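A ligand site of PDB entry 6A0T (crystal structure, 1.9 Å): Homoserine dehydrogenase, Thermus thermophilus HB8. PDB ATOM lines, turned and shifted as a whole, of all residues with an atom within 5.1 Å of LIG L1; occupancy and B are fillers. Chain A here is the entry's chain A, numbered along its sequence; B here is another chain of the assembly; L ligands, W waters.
The side-chain carboxylate (OE2) of Glu 180 lies within hydrogen-bond range of an oxygen (O13) of LIG L1, at 2.7 Å.
An oxygen (O16) of LIG L1 is in hydrogen-bond range of the backbone NH of Asp 45 (2.8 Å).
The backbone NH (N) of Gly 290 lies within hydrogen-bond range of an oxygen (O14) of LIG L1.
N of Gly 11 is in hydrogen-bond range of O5 of LIG L1 (2.8 Å).
An oxygen (O15) of LIG L1 lies within salt-bridge range of the guanidinium group (NH1) of Arg 50 (2.8 Å).
The backbone NH of Arg 44 is in hydrogen-bond range of an oxygen (O16) of LIG L1.
An oxygen (O17) of LIG L1 is in salt-bridge range of the guanidinium group (NH2) of Arg 44, 2.9 Å away.
A nitrogen (N7) of LIG L1 lies within hydrogen-bond range of the backbone carbonyl oxygen (O) of Gly 177 (2.9 Å).
O8 of LIG L1 sits at hydrogen-bond distance from N of Val 14, at 2.9 Å.
An oxygen (O2) of LIG L1 sits at hydrogen-bond distance from the backbone NH (N) of Thr 13 (3.0 Å).
An oxygen (O5) of LIG L1 is in hydrogen-bond range of the backbone NH (N) of Gly 12, at 3.1 Å.
The side-chain amide oxygen (OE1) of Gln 174 of chain B sits at hydrogen-bond distance from a nitrogen (N3) of LIG L1, at 3.1 Å.
The backbone NH of Gly 75 sits close to an oxygen (O12) of LIG L1 (3.4 Å).
A nitrogen (N1) of LG2 L2 lies within salt-bridge range of the side-chain carboxylate (OE1) of Glu 180, at 2.7 Å.
The backbone carbonyl oxygen of Tyr 178 lies within hydrogen-bond range of a nitrogen (N1) of LG2 L2 (2.8 Å).
NH2 of Arg 50 lies within hydrogen-bond range of O of Asp 45, 2.9 Å away.
The guanidinium group (NH1) of Arg 50 lies within hydrogen-bond range of the backbone carbonyl oxygen (O) of Gly 11, at 3.0 Å.
The guanidinium group (NH1) of Arg 44 lies close to the side-chain amide oxygen (OE1) of Gln 174 of chain B.
The backbone carbonyl oxygen of Glu 72 sits at hydrogen-bond distance from the backbone NH of Ala 97, at 3.1 Å.
The backbone NH of Gly 75 lies within hydrogen-bond range of the side-chain carboxylate of Glu 72 (3.4 Å).
ND2 of Asn 98 sits at hydrogen-bond distance from O of Gly 76 (2.9 Å).
OE2 of Glu 72 lies within hydrogen-bond range of N of Met 74, 2.8 Å away.
O of Leu 42 is in hydrogen-bond range of N of Gly 10 (2.9 Å).
Gly 10 touches LIG L1.
Leu 42 touches LIG L1.
Val 43 touches LIG L1.
CE of Lys 48 touches O15 of LIG L1 (3.8 Å).
O of Ala 73 touches C11 of LIG L1, 3.2 Å away.
Met 74 touches LIG L1.
O of Ala 97 touches C21 of LIG L1 (3.1 Å).
Asn 98 touches LIG L1 (CG to O12, 3.3 Å).
Ala 122 touches LIG L1.
Ala 289 touches LIG L1.
OG1 of Thr 294 touches C19 of LIG L1, at 3.0 Å.
CD2 of Leu 170 of chain B touches N3 of LIG L1, at 3.9 Å.
Leu 171 of chain B touches LIG L1 (CG to N4, 3.6 Å).
Of the 36 residues printed, 25 come within 4 Å of LIG L1.
Water W15 lies within hydrogen-bond range of O of Ala 179 and O9 of LIG L1.
Water W12 lies within hydrogen-bond range of OD1 of Asn 98 (2.8 Å), O12 of LIG L1 (2.8 Å) and N of Gly 76 (3.2 Å).
Water W6 lies within hydrogen-bond range of N2 of LIG L1 (2.8 Å) and NE2 of Gln 174 of chain B (2.9 Å).
Water W5 lies within hydrogen-bond range of the side-chain carboxylate (OE1) of Glu 180 (2.8 Å), a nitrogen (N7) of LIG L1 (2.8 Å) and the backbone carbonyl oxygen (O) of Ala 179 (3.3 Å).
Water W14 bridges NH2 of Arg 44 (2.7 Å) and O1 of LIG L1 (3.0 Å).
Water W13 lies within hydrogen-bond range of O3 of LG2 L2 (2.7 Å), OD2 of Asp 191 (2.8 Å), OE1 of Glu 180 (3.1 Å) and O13 of LIG L1 (3.2 Å).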
ATOM      1  N   GLY A  10      -1.266  28.009  12.446  1.00  0.00           N
ATOM      2  CA  GLY A  10       0.004  27.919  11.692  1.00  0.00           C
ATOM      3  C   GLY A  10      -0.138  27.276  10.328  1.00  0.00           C
ATOM      4  O   GLY A  10      -0.820  26.215  10.160  1.00  0.00           O
ATOM      5  N   GLY A  11       0.396  27.940   9.267  1.00  0.00           N
ATOM      6  CA  GLY A  11       0.289  27.503   7.924  1.00  0.00           C
ATOM      7  C   GLY A  11       1.606  27.568   7.204  1.00  0.00           C
ATOM      8  O   GLY A  11       1.714  27.841   5.975  1.00  0.00           O
ATOM      9  N   GLY A  12       2.650  27.199   7.938  1.00  0.00           N
ATOM     10  CA  GLY A  12       3.986  27.208   7.452  1.00  0.00           C
ATOM     11  C   GLY A  12       4.492  25.869   6.973  1.00  0.00           C
ATOM     12  O   GLY A  12       3.776  25.119   6.330  1.00  0.00           O
ATOM     13  N   THR A  13       5.755  25.581   7.191  1.00  0.00           N
ATOM     14  CA  THR A  13       6.381  24.326   6.758  1.00  0.00           C
ATOM     15  C   THR A  13       5.483  23.120   7.229  1.00  0.00           C
ATOM     16  O   THR A  13       5.099  22.295   6.401  1.00  0.00           O
ATOM     17  CB  THR A  13       7.776  24.209   7.356  1.00  0.00           C
ATOM     18  OG1 THR A  13       8.622  25.160   6.667  1.00  0.00           O
ATOM     19  CG2 THR A  13       8.345  22.855   6.918  1.00  0.00           C
ATOM     20  N   VAL A  14       5.198  23.074   8.499  1.00  0.00           N
ATOM     21  CA  VAL A  14       4.414  21.981   9.082  1.00  0.00           C
ATOM     22  C   VAL A  14       2.926  22.199   8.813  1.00  0.00           C
ATOM     23  O   VAL A  14       2.216  21.281   8.331  1.00  0.00           O
ATOM     24  CB  VAL A  14       4.626  21.899  10.568  1.00  0.00           C
ATOM     25  CG1 VAL A  14       3.684  20.885  11.211  1.00  0.00           C
ATOM     26  CG2 VAL A  14       6.075  21.649  10.868  1.00  0.00           C
ATOM     27  N   GLY A  15       2.366  23.387   9.036  1.00  0.00           N
ATOM     28  CA  GLY A  15       0.927  23.554   8.856  1.00  0.00           C
ATOM     29  C   GLY A  15       0.396  23.403   7.472  1.00  0.00           C
ATOM     30  O   GLY A  15      -0.642  22.777   7.252  1.00  0.00           O
ATOM     31  N   LEU A  42      -4.714  29.999  11.009  1.00  0.00           N
ATOM     32  CA  LEU A  42      -4.055  31.266  11.562  1.00  0.00           C
ATOM     33  C   LEU A  42      -2.731  31.389  10.960  1.00  0.00           C
ATOM     34  O   LEU A  42      -1.909  30.449  10.969  1.00  0.00           O
ATOM     35  CB  LEU A  42      -3.918  31.214  13.082  1.00  0.00           C
ATOM     36  CG  LEU A  42      -3.266  32.419  13.781  1.00  0.00           C
ATOM     37  CD1 LEU A  42      -4.193  33.620  13.534  1.00  0.00           C
ATOM     38  CD2 LEU A  42      -3.107  32.092  15.233  1.00  0.00           C
ATOM     39  N   VAL A  43      -2.441  32.571  10.361  1.00  0.00           N
ATOM     40  CA  VAL A  43      -1.159  32.856   9.795  1.00  0.00           C
ATOM     41  C   VAL A  43      -0.871  34.345  10.109  1.00  0.00           C
ATOM     42  O   VAL A  43      -1.713  35.044  10.672  1.00  0.00           O
ATOM     43  CB  VAL A  43      -1.047  32.622   8.298  1.00  0.00           C
ATOM     44  CG1 VAL A  43      -1.397  31.165   7.914  1.00  0.00           C
ATOM     45  CG2 VAL A  43      -1.974  33.628   7.559  1.00  0.00           C
ATOM     46  N   ARG A  44       0.357  34.738   9.859  1.00  0.00           N
ATOM     47  CA  ARG A  44       0.761  36.173  10.121  1.00  0.00           C
ATOM     48  C   ARG A  44       0.485  36.987   8.918  1.00  0.00           C
ATOM     49  O   ARG A  44      -0.132  38.054   9.021  1.00  0.00           O
ATOM     50  CB  ARG A  44       2.290  36.276  10.394  1.00  0.00           C
ATOM     51  CG  ARG A  44       2.632  35.832  11.757  1.00  0.00           C
ATOM     52  CD  ARG A  44       3.962  36.513  12.262  1.00  0.00           C
ATOM     53  NE  ARG A  44       4.910  35.746  11.585  1.00  0.00           N
ATOM     54  CZ  ARG A  44       5.708  34.786  12.022  1.00  0.00           C
ATOM     55  NH1 ARG A  44       6.188  34.663  13.235  1.00  0.00           N
ATOM     56  NH2 ARG A  44       6.257  34.094  11.071  1.00  0.00           N
ATOM     57  N   ASP A  45       0.921  36.481   7.772  1.00  0.00           N
ATOM     58  CA  ASP A  45       0.850  37.233   6.514  1.00  0.00           C
ATOM     59  C   ASP A  45      -0.013  36.559   5.483  1.00  0.00           C
ATOM     60  O   ASP A  45       0.438  35.719   4.719  1.00  0.00           O
ATOM     61  CB  ASP A  45       2.238  37.448   5.967  1.00  0.00           C
ATOM     62  CG  ASP A  45       2.266  38.353   4.686  1.00  0.00           C
ATOM     63  OD1 ASP A  45       3.381  38.551   4.171  1.00  0.00           O
ATOM     64  OD2 ASP A  45       1.178  38.770   4.198  1.00  0.00           O
ATOM     65  N   LYS A  48       1.337  36.153   1.661  1.00  0.00           N
ATOM     66  CA  LYS A  48       2.400  35.300   1.172  1.00  0.00           C
ATOM     67  C   LYS A  48       1.711  34.197   0.247  1.00  0.00           C
ATOM     68  O   LYS A  48       0.621  33.795   0.550  1.00  0.00           O
ATOM     69  CB  LYS A  48       3.048  34.470   2.325  1.00  0.00           C
ATOM     70  CG  LYS A  48       4.150  35.103   3.137  1.00  0.00           C
ATOM     71  CD  LYS A  48       4.491  34.363   4.442  1.00  0.00           C
ATOM     72  CE  LYS A  48       5.298  33.081   4.257  1.00  0.00           C
ATOM     73  NZ  LYS A  48       6.703  33.122   4.844  1.00  0.00           N
ATOM     74  N   ARG A  50       0.755  30.648  -0.781  1.00  0.00           N
ATOM     75  CA  ARG A  50       0.548  29.601   0.221  1.00  0.00           C
ATOM     76  C   ARG A  50      -0.396  28.599  -0.374  1.00  0.00           C
ATOM     77  O   ARG A  50      -1.354  28.962  -1.008  1.00  0.00           O
ATOM     78  CB  ARG A  50      -0.143  30.211   1.433  1.00  0.00           C
ATOM     79  CG  ARG A  50       0.179  29.410   2.733  1.00  0.00           C
ATOM     80  CD  ARG A  50      -0.506  29.939   3.864  1.00  0.00           C
ATOM     81  NE  ARG A  50      -0.132  31.333   4.227  1.00  0.00           N
ATOM     82  CZ  ARG A  50       0.831  31.678   5.061  1.00  0.00           C
ATOM     83  NH1 ARG A  50       1.591  30.785   5.653  1.00  0.00           N
ATOM     84  NH2 ARG A  50       1.063  32.978   5.328  1.00  0.00           N
ATOM     85  N   GLU A  72      -2.141  22.602  16.213  1.00  0.00           N
ATOM     86  CA  GLU A  72      -1.189  23.692  16.391  1.00  0.00           C
ATOM     87  C   GLU A  72       0.222  23.390  15.917  1.00  0.00           C
ATOM     88  O   GLU A  72       0.881  22.423  16.330  1.00  0.00           O
ATOM     89  CB  GLU A  72      -1.233  24.272  17.812  1.00  0.00           C
ATOM     90  CG  GLU A  72      -0.269  25.494  18.015  1.00  0.00           C
ATOM     91  CD  GLU A  72       1.173  25.161  18.336  1.00  0.00           C
ATOM     92  OE1 GLU A  72       1.291  24.306  19.239  1.00  0.00           O
ATOM     93  OE2 GLU A  72       2.135  25.869  17.865  1.00  0.00           O
ATOM     94  N   ALA A  73       0.773  24.287  15.056  1.00  0.00           N
ATOM     95  CA  ALA A  73       2.143  24.278  14.624  1.00  0.00           C
ATOM     96  C   ALA A  73       2.546  25.723  14.217  1.00  0.00           C
ATOM     97  O   ALA A  73       2.871  25.988  13.091  1.00  0.00           O
ATOM     98  CB  ALA A  73       2.356  23.342  13.492  1.00  0.00           C
ATOM     99  N   MET A  74       2.414  26.589  15.187  1.00  0.00           N
ATOM    100  CA  MET A  74       2.707  28.063  14.919  1.00  0.00           C
ATOM    101  C   MET A  74       4.030  28.464  15.511  1.00  0.00           C
ATOM    102  O   MET A  74       4.567  29.485  15.145  1.00  0.00           O
ATOM    103  CB  MET A  74       1.521  28.924  15.395  1.00  0.00           C
ATOM    104  CG  MET A  74       1.353  29.046  16.844  1.00  0.00           C
ATOM    105  SD  MET A  74      -0.103  29.989  17.354  1.00  0.00           S
ATOM    106  CE  MET A  74       0.522  31.661  16.967  1.00  0.00           C
ATOM    107  N   GLY A  75       4.618  27.683  16.434  1.00  0.00           N
ATOM    108  CA  GLY A  75       5.832  28.041  17.085  1.00  0.00           C
ATOM    109  C   GLY A  75       5.611  29.055  18.248  1.00  0.00           C
ATOM    110  O   GLY A  75       4.525  29.633  18.512  1.00  0.00           O
ATOM    111  N   GLY A  76       6.627  29.114  19.090  1.00  0.00           N
ATOM    112  CA  GLY A  76       6.661  29.914  20.315  1.00  0.00           C
ATOM    113  C   GLY A  76       5.878  29.260  21.431  1.00  0.00           C
ATOM    114  O   GLY A  76       5.606  28.040  21.362  1.00  0.00           O
ATOM    115  N   ALA A  79       1.958  32.677  22.937  1.00  0.00           N
ATOM    116  CA  ALA A  79       0.833  32.893  22.022  1.00  0.00           C
ATOM    117  C   ALA A  79       0.008  31.609  21.742  1.00  0.00           C
ATOM    118  O   ALA A  79      -1.224  31.608  21.931  1.00  0.00           O
ATOM    119  CB  ALA A  79       1.284  33.533  20.724  1.00  0.00           C
ATOM    120  N   ALA A  97       2.499  19.970  17.304  1.00  0.00           N
ATOM    121  CA  ALA A  97       3.914  19.645  17.030  1.00  0.00           C
ATOM    122  C   ALA A  97       4.919  20.454  17.806  1.00  0.00           C
ATOM    123  O   ALA A  97       6.140  20.394  17.570  1.00  0.00           O
ATOM    124  CB  ALA A  97       4.191  19.803  15.541  1.00  0.00           C
ATOM    125  N   ASN A  98       4.431  21.205  18.747  1.00  0.00           N
ATOM    126  CA  ASN A  98       5.294  22.284  19.402  1.00  0.00           C
ATOM    127  C   ASN A  98       5.844  21.835  20.768  1.00  0.00           C
ATOM    128  O   ASN A  98       5.191  21.955  21.813  1.00  0.00           O
ATOM    129  CB  ASN A  98       4.398  23.483  19.548  1.00  0.00           C
ATOM    130  CG  ASN A  98       5.149  24.754  19.917  1.00  0.00           C
ATOM    131  OD1 ASN A  98       6.264  24.711  20.510  1.00  0.00           O
ATOM    132  ND2 ASN A  98       4.483  25.880  19.698  1.00  0.00           N
ATOM    133  N   ALA A 122       3.971  14.451  16.974  1.00  0.00           N
ATOM    134  CA  ALA A 122       4.825  15.177  16.032  1.00  0.00           C
ATOM    135  C   ALA A 122       5.817  16.107  16.713  1.00  0.00           C
ATOM    136  O   ALA A 122       6.668  16.682  16.066  1.00  0.00           O
ATOM    137  CB  ALA A 122       3.946  16.000  15.081  1.00  0.00           C
ATOM    138  N   ALA A 126       9.181  14.150  14.833  1.00  0.00           N
ATOM    139  CA  ALA A 126       8.230  14.329  13.718  1.00  0.00           C
ATOM    140  C   ALA A 126       7.333  13.082  13.685  1.00  0.00           C
ATOM    141  O   ALA A 126       6.867  12.649  14.768  1.00  0.00           O
ATOM    142  CB  ALA A 126       8.924  14.558  12.397  1.00  0.00           C
ATOM    143  N   GLY A 177      13.668  22.720   5.454  1.00  0.00           N
ATOM    144  CA  GLY A 177      12.590  23.074   6.318  1.00  0.00           C
ATOM    145  C   GLY A 177      12.800  22.537   7.717  1.00  0.00           C
ATOM    146  O   GLY A 177      11.837  22.434   8.468  1.00  0.00           O
ATOM    147  N   TYR A 178      14.012  22.161   8.072  1.00  0.00           N
ATOM    148  CA  TYR A 178      14.230  21.481   9.381  1.00  0.00           C
ATOM    149  C   TYR A 178      14.330  22.432  10.576  1.00  0.00           C
ATOM    150  O   TYR A 178      14.077  22.044  11.697  1.00  0.00           O
ATOM    151  CB  TYR A 178      15.501  20.641   9.405  1.00  0.00           C
ATOM    152  CG  TYR A 178      15.584  19.543   8.402  1.00  0.00           C
ATOM    153  CD1 TYR A 178      14.442  18.991   7.778  1.00  0.00           C
ATOM    154  CD2 TYR A 178      16.805  18.996   8.084  1.00  0.00           C
ATOM    155  CE1 TYR A 178      14.542  17.901   6.895  1.00  0.00           C
ATOM    156  CE2 TYR A 178      16.910  17.992   7.151  1.00  0.00           C
ATOM    157  CZ  TYR A 178      15.764  17.478   6.552  1.00  0.00           C
ATOM    158  OH  TYR A 178      15.928  16.469   5.661  1.00  0.00           O
ATOM    159  N   ALA A 179      14.841  23.678  10.363  1.00  0.00           N
ATOM    160  CA  ALA A 179      15.336  24.478  11.508  1.00  0.00           C
ATOM    161  C   ALA A 179      14.272  25.282  12.153  1.00  0.00           C
ATOM    162  O   ALA A 179      13.326  25.689  11.483  1.00  0.00           O
ATOM    163  CB  ALA A 179      16.427  25.443  10.992  1.00  0.00           C
ATOM    164  N   GLU A 180      14.436  25.567  13.429  1.00  0.00           N
ATOM    165  CA  GLU A 180      13.609  26.580  14.039  1.00  0.00           C
ATOM    166  C   GLU A 180      13.844  27.973  13.424  1.00  0.00           C
ATOM    167  O   GLU A 180      14.865  28.166  12.788  1.00  0.00           O
ATOM    168  CB  GLU A 180      13.903  26.617  15.531  1.00  0.00           C
ATOM    169  CG  GLU A 180      13.628  25.323  16.296  1.00  0.00           C
ATOM    170  CD  GLU A 180      12.212  24.875  16.066  1.00  0.00           C
ATOM    171  OE1 GLU A 180      12.080  23.790  15.427  1.00  0.00           O
ATOM    172  OE2 GLU A 180      11.273  25.543  16.465  1.00  0.00           O
ATOM    173  N   ASP A 191      16.168  22.985  21.577  1.00  0.00           N
ATOM    174  CA  ASP A 191      15.094  22.169  20.992  1.00  0.00           C
ATOM    175  C   ASP A 191      15.188  20.696  21.505  1.00  0.00           C
ATOM    176  O   ASP A 191      14.185  20.132  21.938  1.00  0.00           O
ATOM    177  CB  ASP A 191      15.117  22.282  19.489  1.00  0.00           C
ATOM    178  CG  ASP A 191      14.091  21.305  18.817  1.00  0.00           C
ATOM    179  OD1 ASP A 191      14.600  20.236  18.422  1.00  0.00           O
ATOM    180  OD2 ASP A 191      12.899  21.676  18.844  1.00  0.00           O
ATOM    181  N   GLY A 288      13.384  13.089  11.586  1.00  0.00           N
ATOM    182  CA  GLY A 288      13.004  13.879  12.731  1.00  0.00           C
ATOM    183  C   GLY A 288      12.631  15.320  12.505  1.00  0.00           C
ATOM    184  O   GLY A 288      12.292  16.005  13.478  1.00  0.00           O
ATOM    185  N   ALA A 289      12.526  15.679  11.232  1.00  0.00           N
ATOM    186  CA  ALA A 289      12.112  17.015  10.896  1.00  0.00           C
ATOM    187  C   ALA A 289      11.671  16.999   9.447  1.00  0.00           C
ATOM    188  O   ALA A 289      11.908  16.025   8.704  1.00  0.00           O
ATOM    189  CB  ALA A 289      13.310  17.929  11.081  1.00  0.00           C
ATOM    190  N   GLY A 290      11.077  18.124   9.026  1.00  0.00           N
ATOM    191  CA  GLY A 290      10.588  18.216   7.657  1.00  0.00           C
ATOM    192  C   GLY A 290       9.082  18.280   7.605  1.00  0.00           C
ATOM    193  O   GLY A 290       8.423  17.729   8.484  1.00  0.00           O
ATOM    194  N   GLY A 291       8.529  19.025   6.653  1.00  0.00           N
ATOM    195  CA  GLY A 291       7.091  19.224   6.660  1.00  0.00           C
ATOM    196  C   GLY A 291       6.282  17.930   6.539  1.00  0.00           C
ATOM    197  O   GLY A 291       5.397  17.722   7.318  1.00  0.00           O
ATOM    198  N   THR A 294       6.515  15.663   9.555  1.00  0.00           N
ATOM    199  CA  THR A 294       5.804  16.144  10.653  1.00  0.00           C
ATOM    200  C   THR A 294       4.304  16.009  10.442  1.00  0.00           C
ATOM    201  O   THR A 294       3.494  15.668  11.337  1.00  0.00           O
ATOM    202  CB  THR A 294       6.246  17.586  11.022  1.00  0.00           C
ATOM    203  OG1 THR A 294       7.646  17.592  11.066  1.00  0.00           O
ATOM    204  CG2 THR A 294       5.586  18.050  12.274  1.00  0.00           C
ATOM    205  N   ALA B 167      -2.103  37.576  21.805  1.00  0.00           N
ATOM    206  CA  ALA B 167      -1.720  36.963  20.529  1.00  0.00           C
ATOM    207  C   ALA B 167      -1.877  37.881  19.314  1.00  0.00           C
ATOM    208  O   ALA B 167      -1.098  37.821  18.394  1.00  0.00           O
ATOM    209  CB  ALA B 167      -2.524  35.655  20.254  1.00  0.00           C
ATOM    210  N   LEU B 170       1.220  40.369  19.638  1.00  0.00           N
ATOM    211  CA  LEU B 170       2.450  39.697  19.181  1.00  0.00           C
ATOM    212  C   LEU B 170       2.580  39.584  17.717  1.00  0.00           C
ATOM    213  O   LEU B 170       3.607  39.897  17.096  1.00  0.00           O
ATOM    214  CB  LEU B 170       2.657  38.360  19.920  1.00  0.00           C
ATOM    215  CG  LEU B 170       3.884  37.602  19.391  1.00  0.00           C
ATOM    216  CD1 LEU B 170       5.241  38.225  19.793  1.00  0.00           C
ATOM    217  CD2 LEU B 170       3.883  36.154  19.797  1.00  0.00           C
ATOM    218  N   LEU B 171       1.501  39.131  17.046  1.00  0.00           N
ATOM    219  CA  LEU B 171       1.517  39.010  15.616  1.00  0.00           C
ATOM    220  C   LEU B 171       1.870  40.372  14.951  1.00  0.00           C
ATOM    221  O   LEU B 171       2.661  40.461  14.017  1.00  0.00           O
ATOM    222  CB  LEU B 171       0.066  38.584  15.190  1.00  0.00           C
ATOM    223  CG  LEU B 171      -0.195  38.016  13.811  1.00  0.00           C
ATOM    224  CD1 LEU B 171      -1.697  37.605  13.789  1.00  0.00           C
ATOM    225  CD2 LEU B 171       0.059  39.116  12.860  1.00  0.00           C
ATOM    226  N   GLN B 174       5.529  41.332  15.374  1.00  0.00           N
ATOM    227  CA  GLN B 174       6.328  40.592  14.456  1.00  0.00           C
ATOM    228  C   GLN B 174       6.231  41.168  13.027  1.00  0.00           C
ATOM    229  O   GLN B 174       7.270  41.334  12.335  1.00  0.00           O
ATOM    230  CB  GLN B 174       5.940  39.062  14.454  1.00  0.00           C
ATOM    231  CG  GLN B 174       6.224  38.384  15.775  1.00  0.00           C
ATOM    232  CD  GLN B 174       5.695  36.965  15.815  1.00  0.00           C
ATOM    233  OE1 GLN B 174       4.579  36.703  15.397  1.00  0.00           O
ATOM    234  NE2 GLN B 174       6.399  36.116  16.461  1.00  0.00           N
HETATM  235  P1  LIG L   1       7.040  28.058  10.134  1.00  0.00           P
HETATM  236  O1  LIG L   1       7.738  29.315  10.589  1.00  0.00           O
HETATM  237  O2  LIG L   1       7.245  27.608   8.831  1.00  0.00           O
HETATM  238  O3  LIG L   1       5.508  28.333  10.305  1.00  0.00           O
HETATM  239  C1  LIG L   1       4.906  29.021  11.404  1.00  0.00           C
HETATM  240  C2  LIG L   1       3.503  29.405  11.004  1.00  0.00           C
HETATM  241  O4  LIG L   1       2.837  30.026  12.032  1.00  0.00           O
HETATM  242  C3  LIG L   1       3.444  30.344   9.768  1.00  0.00           C
HETATM  243  O5  LIG L   1       2.212  30.068   9.049  1.00  0.00           O
HETATM  244  C4  LIG L   1       3.397  31.741  10.460  1.00  0.00           C
HETATM  245  O6  LIG L   1       2.688  32.716   9.709  1.00  0.00           O
HETATM  246  C5  LIG L   1       2.532  31.403  11.646  1.00  0.00           C
HETATM  247  N1  LIG L   1       2.697  32.249  12.840  1.00  0.00           N
HETATM  248  C6  LIG L   1       3.833  32.340  13.589  1.00  0.00           C
HETATM  249  N2  LIG L   1       3.693  33.165  14.646  1.00  0.00           N
HETATM  250  C7  LIG L   1       2.390  33.570  14.540  1.00  0.00           C
HETATM  251  C8  LIG L   1       1.593  34.440  15.343  1.00  0.00           C
HETATM  252  N3  LIG L   1       2.149  35.057  16.436  1.00  0.00           N
HETATM  253  N4  LIG L   1       0.350  34.658  15.012  1.00  0.00           N
HETATM  254  C9  LIG L   1      -0.249  34.043  13.934  1.00  0.00           C
HETATM  255  N5  LIG L   1       0.427  33.226  13.113  1.00  0.00           N
HETATM  256  C10 LIG L   1       1.725  32.973  13.402  1.00  0.00           C
HETATM  257  O7  LIG L   1       7.405  27.100  11.307  1.00  0.00           O
HETATM  258  P2  LIG L   1       7.318  25.421  11.166  1.00  0.00           P
HETATM  259  O8  LIG L   1       6.116  25.095  10.426  1.00  0.00           O
HETATM  260  O9  LIG L   1       8.607  24.946  10.716  1.00  0.00           O
HETATM  261  O10 LIG L   1       7.205  25.005  12.693  1.00  0.00           O
HETATM  262  C11 LIG L   1       5.975  25.174  13.401  1.00  0.00           C
HETATM  263  C12 LIG L   1       5.984  24.480  14.745  1.00  0.00           C
HETATM  264  O11 LIG L   1       6.312  23.073  14.555  1.00  0.00           O
HETATM  265  C13 LIG L   1       7.155  25.016  15.647  1.00  0.00           C
HETATM  266  O12 LIG L   1       6.598  24.929  16.968  1.00  0.00           O
HETATM  267  C14 LIG L   1       8.326  24.082  15.429  1.00  0.00           C
HETATM  268  O13 LIG L   1       9.120  23.921  16.577  1.00  0.00           O
HETATM  269  C15 LIG L   1       7.511  22.776  15.297  1.00  0.00           C
HETATM  270  N6  LIG L   1       8.094  21.717  14.519  1.00  0.00           N
HETATM  271  C16 LIG L   1       8.760  21.909  13.340  1.00  0.00           C
HETATM  272  C17 LIG L   1       9.187  20.888  12.556  1.00  0.00           C
HETATM  273  C18 LIG L   1       9.973  21.064  11.309  1.00  0.00           C
HETATM  274  O14 LIG L   1      10.617  20.132  10.874  1.00  0.00           O
HETATM  275  N7  LIG L   1       9.994  22.264  10.686  1.00  0.00           N
HETATM  276  C19 LIG L   1       8.900  19.555  12.963  1.00  0.00           C
HETATM  277  C20 LIG L   1       8.234  19.363  14.142  1.00  0.00           C
HETATM  278  C21 LIG L   1       7.810  20.430  14.921  1.00  0.00           C
HETATM  279  P3  LIG L   1       3.376  33.148   8.273  1.00  0.00           P
HETATM  280  O15 LIG L   1       3.479  31.972   7.389  1.00  0.00           O
HETATM  281  O16 LIG L   1       2.302  34.094   7.850  1.00  0.00           O
HETATM  282  O17 LIG L   1       4.607  33.792   8.704  1.00  0.00           O
HETATM  283  N1  LG2 L   2      14.100  22.219  14.501  1.00  0.00           N
HETATM  284  C1  LG2 L   2      13.630  20.841  14.813  1.00  0.00           C
HETATM  285  C2  LG2 L   2      14.758  19.885  14.618  1.00  0.00           C
HETATM  286  C3  LG2 L   2      12.490  20.487  13.879  1.00  0.00           C
HETATM  287  O1  LG2 L   2      15.770  20.160  13.872  1.00  0.00           O
HETATM  288  O2  LG2 L   2      14.752  18.738  15.164  1.00  0.00           O
HETATM  289  C4  LG2 L   2      11.877  19.103  14.270  1.00  0.00           C
HETATM  290  O3  LG2 L   2      11.256  19.006  15.567  1.00  0.00           O
HETATM  291  O   HOH W   1       7.245  31.918   8.838  1.00  0.00           O
HETATM  292  O   HOH W   2      10.483  28.486  10.669  1.00  0.00           O
HETATM  293  O   HOH W   3       5.485  30.638   6.139  1.00  0.00           O
HETATM  294  O   HOH W   4       9.201  23.335  19.439  1.00  0.00           O
HETATM  295  O   HOH W   5      10.990  23.778  12.873  1.00  0.00           O
HETATM  296  O   HOH W   6       5.514  33.332  16.811  1.00  0.00           O
HETATM  297  O   HOH W   7       3.403  25.698  10.394  1.00  0.00           O
HETATM  298  O   HOH W   8       8.278  28.174  13.911  1.00  0.00           O
HETATM  299  O   HOH W   9      11.594  25.285   9.196  1.00  0.00           O
HETATM  300  O   HOH W  10      -0.597  35.255  17.628  1.00  0.00           O
HETATM  301  O   HOH W  11       7.442  28.990   6.664  1.00  0.00           O
HETATM  302  O   HOH W  12       8.017  26.257  19.007  1.00  0.00           O
HETATM  303  O   HOH W  13      10.914  21.317  16.900  1.00  0.00           O
HETATM  304  O   HOH W  14       7.332  31.834  12.078  1.00  0.00           O
HETATM  305  O   HOH W  15      10.754  26.175  11.815  1.00  0.00           O
HETATM  306  O   HOH W  16       5.298  36.309   8.070  1.00  0.00           O
